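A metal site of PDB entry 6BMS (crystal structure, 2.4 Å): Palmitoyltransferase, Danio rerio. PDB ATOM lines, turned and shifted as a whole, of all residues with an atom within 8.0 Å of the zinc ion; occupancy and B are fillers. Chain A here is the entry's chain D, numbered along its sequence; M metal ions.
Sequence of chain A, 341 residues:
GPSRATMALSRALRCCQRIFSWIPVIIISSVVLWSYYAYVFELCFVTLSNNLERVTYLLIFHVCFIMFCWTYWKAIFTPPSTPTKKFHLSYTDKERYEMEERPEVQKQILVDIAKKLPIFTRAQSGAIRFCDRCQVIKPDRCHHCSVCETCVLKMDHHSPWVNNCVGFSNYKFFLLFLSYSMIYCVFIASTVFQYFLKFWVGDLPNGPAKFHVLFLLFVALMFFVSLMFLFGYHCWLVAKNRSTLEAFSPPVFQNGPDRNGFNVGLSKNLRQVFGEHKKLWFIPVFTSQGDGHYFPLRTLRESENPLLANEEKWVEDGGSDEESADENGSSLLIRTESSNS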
ATOM      1  N   PRO A  83      19.793   7.492 -18.332  1.00  0.00           N
ATOM      2  CA  PRO A  83      19.558   6.340 -19.197  1.00  0.00           C
ATOM      3  C   PRO A  83      19.911   6.622 -20.646  1.00  0.00           C
ATOM      4  O   PRO A  83      19.682   7.712 -21.173  1.00  0.00           O
ATOM      5  CB  PRO A  83      18.060   6.069 -19.031  1.00  0.00           C
ATOM      6  CG  PRO A  83      17.770   6.517 -17.651  1.00  0.00           C
ATOM      7  CD  PRO A  83      18.661   7.710 -17.401  1.00  0.00           C
ATOM      8  N   HIS A  88      14.906   4.975 -23.494  1.00  0.00           N
ATOM      9  CA  HIS A  88      13.864   5.969 -23.725  1.00  0.00           C
ATOM     10  C   HIS A  88      12.806   5.402 -24.678  1.00  0.00           C
ATOM     11  O   HIS A  88      13.128   4.722 -25.650  1.00  0.00           O
ATOM     12  CB  HIS A  88      14.448   7.243 -24.314  1.00  0.00           C
ATOM     13  CG  HIS A  88      15.152   8.107 -23.326  1.00  0.00           C
ATOM     14  ND1 HIS A  88      16.373   7.775 -22.773  1.00  0.00           N
ATOM     15  CD2 HIS A  88      14.818   9.313 -22.801  1.00  0.00           C
ATOM     16  CE1 HIS A  88      16.751   8.727 -21.932  1.00  0.00           C
ATOM     17  NE2 HIS A  88      15.826   9.677 -21.936  1.00  0.00           N
ATOM     18  N   PHE A 130       8.662   2.501 -14.704  1.00  0.00           N
ATOM     19  CA  PHE A 130       8.490   3.460 -15.788  1.00  0.00           C
ATOM     20  C   PHE A 130       8.428   4.868 -15.212  1.00  0.00           C
ATOM     21  O   PHE A 130       7.819   5.093 -14.158  1.00  0.00           O
ATOM     22  CB  PHE A 130       7.212   3.153 -16.576  1.00  0.00           C
ATOM     23  CG  PHE A 130       6.945   4.126 -17.703  1.00  0.00           C
ATOM     24  CD1 PHE A 130       7.754   4.154 -18.821  1.00  0.00           C
ATOM     25  CD2 PHE A 130       5.866   4.991 -17.642  1.00  0.00           C
ATOM     26  CE1 PHE A 130       7.508   5.040 -19.858  1.00  0.00           C
ATOM     27  CE2 PHE A 130       5.606   5.881 -18.680  1.00  0.00           C
ATOM     28  CZ  PHE A 130       6.432   5.900 -19.790  1.00  0.00           C
ATOM     29  N   CYS A 131       9.071   5.803 -15.890  1.00  0.00           N
ATOM     30  CA  CYS A 131       9.052   7.206 -15.518  1.00  0.00           C
ATOM     31  C   CYS A 131       8.232   7.975 -16.556  1.00  0.00           C
ATOM     32  O   CYS A 131       8.647   8.093 -17.709  1.00  0.00           O
ATOM     33  CB  CYS A 131      10.467   7.773 -15.417  1.00  0.00           C
ATOM     34  SG  CYS A 131      10.530   9.498 -14.870  1.00  0.00           S
ATOM     35  N   ASP A 132       7.070   8.479 -16.139  1.00  0.00           N
ATOM     36  CA  ASP A 132       6.231   9.240 -17.063  1.00  0.00           C
ATOM     37  C   ASP A 132       6.854  10.582 -17.419  1.00  0.00           C
ATOM     38  O   ASP A 132       6.635  11.087 -18.532  1.00  0.00           O
ATOM     39  CB  ASP A 132       4.837   9.444 -16.463  1.00  0.00           C
ATOM     40  CG  ASP A 132       4.892   9.901 -15.015  1.00  0.00           C
ATOM     41  OD1 ASP A 132       5.923  10.465 -14.597  1.00  0.00           O
ATOM     42  OD2 ASP A 132       3.888   9.705 -14.292  1.00  0.00           O
ATOM     43  N   ARG A 133       7.631  11.163 -16.513  1.00  0.00           N
ATOM     44  CA  ARG A 133       8.169  12.504 -16.747  1.00  0.00           C
ATOM     45  C   ARG A 133       9.309  12.467 -17.765  1.00  0.00           C
ATOM     46  O   ARG A 133       9.410  13.359 -18.616  1.00  0.00           O
ATOM     47  CB  ARG A 133       8.628  13.122 -15.427  1.00  0.00           C
ATOM     48  CG  ARG A 133       7.464  13.534 -14.525  1.00  0.00           C
ATOM     49  CD  ARG A 133       7.915  13.834 -13.106  1.00  0.00           C
ATOM     50  NE  ARG A 133       8.168  12.621 -12.342  1.00  0.00           N
ATOM     51  CZ  ARG A 133       8.409  12.600 -11.035  1.00  0.00           C
ATOM     52  NH1 ARG A 133       8.424  13.732 -10.335  1.00  0.00           N
ATOM     53  NH2 ARG A 133       8.630  11.454 -10.416  1.00  0.00           N
ATOM     54  N   CYS A 134      10.173  11.456 -17.682  1.00  0.00           N
ATOM     55  CA  CYS A 134      11.234  11.278 -18.664  1.00  0.00           C
ATOM     56  C   CYS A 134      10.825  10.409 -19.836  1.00  0.00           C
ATOM     57  O   CYS A 134      11.566  10.346 -20.836  1.00  0.00           O
ATOM     58  CB  CYS A 134      12.487  10.689 -18.000  1.00  0.00           C
ATOM     59  SG  CYS A 134      13.194  11.697 -16.685  1.00  0.00           S
ATOM     60  N   GLN A 135       9.674   9.742 -19.758  1.00  0.00           N
ATOM     61  CA  GLN A 135       9.251   8.745 -20.745  1.00  0.00           C
ATOM     62  C   GLN A 135      10.332   7.680 -20.927  1.00  0.00           C
ATOM     63  O   GLN A 135      10.818   7.417 -22.034  1.00  0.00           O
ATOM     64  CB  GLN A 135       8.902   9.423 -22.081  1.00  0.00           C
ATOM     65  CG  GLN A 135       7.615  10.233 -22.045  1.00  0.00           C
ATOM     66  CD  GLN A 135       6.395   9.384 -21.731  1.00  0.00           C
ATOM     67  OE1 GLN A 135       6.036   8.483 -22.493  1.00  0.00           O
ATOM     68  NE2 GLN A 135       5.760   9.658 -20.600  1.00  0.00           N
ATOM     69  N   VAL A 136      10.704   7.072 -19.803  1.00  0.00           N
ATOM     70  CA  VAL A 136      11.867   6.202 -19.730  1.00  0.00           C
ATOM     71  C   VAL A 136      11.477   4.904 -19.042  1.00  0.00           C
ATOM     72  O   VAL A 136      10.850   4.929 -17.973  1.00  0.00           O
ATOM     73  CB  VAL A 136      13.039   6.875 -18.976  1.00  0.00           C
ATOM     74  CG1 VAL A 136      13.940   5.841 -18.328  1.00  0.00           C
ATOM     75  CG2 VAL A 136      13.832   7.762 -19.913  1.00  0.00           C
ATOM     76  N   LYS A 138      12.932   2.376 -16.861  1.00  0.00           N
ATOM     77  CA  LYS A 138      14.075   2.640 -16.000  1.00  0.00           C
ATOM     78  C   LYS A 138      15.040   1.460 -15.989  1.00  0.00           C
ATOM     79  O   LYS A 138      14.613   0.317 -15.792  1.00  0.00           O
ATOM     80  CB  LYS A 138      13.604   2.954 -14.582  1.00  0.00           C
ATOM     81  CG  LYS A 138      12.913   4.296 -14.442  1.00  0.00           C
ATOM     82  CD  LYS A 138      12.648   4.622 -12.976  1.00  0.00           C
ATOM     83  CE  LYS A 138      11.226   4.268 -12.588  1.00  0.00           C
ATOM     84  NZ  LYS A 138      10.702   5.180 -11.536  1.00  0.00           N
ATOM     85  N   CYS A 142      18.172   2.557 -11.326  1.00  0.00           N
ATOM     86  CA  CYS A 142      17.986   3.936 -11.742  1.00  0.00           C
ATOM     87  C   CYS A 142      16.707   4.507 -11.149  1.00  0.00           C
ATOM     88  O   CYS A 142      15.663   3.832 -11.155  1.00  0.00           O
ATOM     89  CB  CYS A 142      17.954   4.047 -13.270  1.00  0.00           C
ATOM     90  SG  CYS A 142      17.308   5.626 -13.894  1.00  0.00           S
ATOM     91  N   HIS A 143      16.777   5.732 -10.635  1.00  0.00           N
ATOM     92  CA  HIS A 143      15.622   6.340  -9.989  1.00  0.00           C
ATOM     93  C   HIS A 143      15.498   7.799 -10.408  1.00  0.00           C
ATOM     94  O   HIS A 143      16.490   8.490 -10.626  1.00  0.00           O
ATOM     95  CB  HIS A 143      15.706   6.256  -8.459  1.00  0.00           C
ATOM     96  CG  HIS A 143      15.689   4.848  -7.938  1.00  0.00           C
ATOM     97  ND1 HIS A 143      14.556   4.259  -7.420  1.00  0.00           N
ATOM     98  CD2 HIS A 143      16.677   3.931  -7.843  1.00  0.00           C
ATOM     99  CE1 HIS A 143      14.844   3.025  -7.036  1.00  0.00           C
ATOM    100  NE2 HIS A 143      16.119   2.800  -7.280  1.00  0.00           N
ATOM    101  N   HIS A 144      14.256   8.267 -10.486  1.00  0.00           N
ATOM    102  CA  HIS A 144      14.002   9.654 -10.878  1.00  0.00           C
ATOM    103  C   HIS A 144      14.233  10.584  -9.691  1.00  0.00           C
ATOM    104  O   HIS A 144      13.700  10.371  -8.601  1.00  0.00           O
ATOM    105  CB  HIS A 144      12.577   9.824 -11.402  1.00  0.00           C
ATOM    106  CG  HIS A 144      12.292  11.207 -11.897  1.00  0.00           C
ATOM    107  ND1 HIS A 144      12.356  11.550 -13.236  1.00  0.00           N
ATOM    108  CD2 HIS A 144      11.939  12.340 -11.240  1.00  0.00           C
ATOM    109  CE1 HIS A 144      12.061  12.828 -13.377  1.00  0.00           C
ATOM    110  NE2 HIS A 144      11.799  13.327 -12.185  1.00  0.00           N
ATOM    111  N   CYS A 145      15.033  11.616  -9.921  1.00  0.00           N
ATOM    112  CA  CYS A 145      15.199  12.704  -8.972  1.00  0.00           C
ATOM    113  C   CYS A 145      14.372  13.899  -9.434  1.00  0.00           C
ATOM    114  O   CYS A 145      14.552  14.378 -10.565  1.00  0.00           O
ATOM    115  CB  CYS A 145      16.669  13.090  -8.815  1.00  0.00           C
ATOM    116  SG  CYS A 145      16.948  14.318  -7.529  1.00  0.00           S
ATOM    117  N   SER A 146      13.473  14.357  -8.558  1.00  0.00           N
ATOM    118  CA  SER A 146      12.620  15.501  -8.850  1.00  0.00           C
ATOM    119  C   SER A 146      13.328  16.824  -8.656  1.00  0.00           C
ATOM    120  O   SER A 146      12.859  17.845  -9.166  1.00  0.00           O
ATOM    121  CB  SER A 146      11.369  15.450  -7.971  1.00  0.00           C
ATOM    122  OG  SER A 146      11.717  15.420  -6.595  1.00  0.00           O
ATOM    123  N   GLU A 149      15.473  16.690 -11.673  1.00  0.00           N
ATOM    124  CA  GLU A 149      14.484  16.606 -12.740  1.00  0.00           C
ATOM    125  C   GLU A 149      14.906  15.632 -13.837  1.00  0.00           C
ATOM    126  O   GLU A 149      14.796  15.920 -15.027  1.00  0.00           O
ATOM    127  CB  GLU A 149      14.190  17.983 -13.341  1.00  0.00           C
ATOM    128  CG  GLU A 149      13.526  18.955 -12.379  1.00  0.00           C
ATOM    129  CD  GLU A 149      13.135  20.257 -13.041  1.00  0.00           C
ATOM    130  OE1 GLU A 149      12.160  20.900 -12.585  1.00  0.00           O
ATOM    131  OE2 GLU A 149      13.804  20.650 -14.018  1.00  0.00           O
ATOM    132  N   THR A 150      15.393  14.452 -13.424  1.00  0.00           N
ATOM    133  CA  THR A 150      15.813  13.474 -14.415  1.00  0.00           C
ATOM    134  C   THR A 150      15.990  12.117 -13.744  1.00  0.00           C
ATOM    135  O   THR A 150      16.164  12.027 -12.528  1.00  0.00           O
ATOM    136  CB  THR A 150      17.120  13.864 -15.118  1.00  0.00           C
ATOM    137  OG1 THR A 150      17.436  12.884 -16.113  1.00  0.00           O
ATOM    138  CG2 THR A 150      18.258  13.936 -14.122  1.00  0.00           C
ATOM    139  N   CYS A 151      15.944  11.068 -14.559  1.00  0.00           N
ATOM    140  CA  CYS A 151      16.296   9.743 -14.089  1.00  0.00           C
ATOM    141  C   CYS A 151      17.803   9.643 -13.926  1.00  0.00           C
ATOM    142  O   CYS A 151      18.573  10.116 -14.766  1.00  0.00           O
ATOM    143  CB  CYS A 151      15.786   8.669 -15.054  1.00  0.00           C
ATOM    144  SG  CYS A 151      14.083   8.154 -14.718  1.00  0.00           S
ATOM    145  N   VAL A 152      18.232   9.041 -12.823  1.00  0.00           N
ATOM    146  CA  VAL A 152      19.631   9.036 -12.390  1.00  0.00           C
ATOM    147  C   VAL A 152      20.074   7.590 -12.234  1.00  0.00           C
ATOM    148  O   VAL A 152      19.408   6.802 -11.542  1.00  0.00           O
ATOM    149  CB  VAL A 152      19.816   9.822 -11.087  1.00  0.00           C
ATOM    150  CG1 VAL A 152      21.247   9.689 -10.580  1.00  0.00           C
ATOM    151  CG2 VAL A 152      19.460  11.287 -11.290  1.00  0.00           C
HETATM  152 ZN    ZN M   1      12.770  10.237 -14.835  1.00  0.00          ZN
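The backbone NH (N) of Arg 133 sits close to the side-chain sulfur (SG) of Cys 131 (3.7 Å).
N of Cys 131 sits at hydrogen-bond distance from O of Val 136.
N of Cys 145 sits at hydrogen-bond distance from O of Thr 150 (2.9 Å).
The zinc ion is bound by a ring nitrogen (ND1) of His 144 (2.1 Å), the side-chain sulfur of Cys 131 (2.4 Å), the side-chain sulfur of Cys 134 (2.4 Å) and the side-chain sulfur of Cys 151 (2.5 Å).
C of Thr 150 touches the zinc ion (3.9 Å).
Five residues have an atom within 4 Å of the zinc ion: Cys 131, Cys 134, His 144, Thr 150 and Cys 151.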
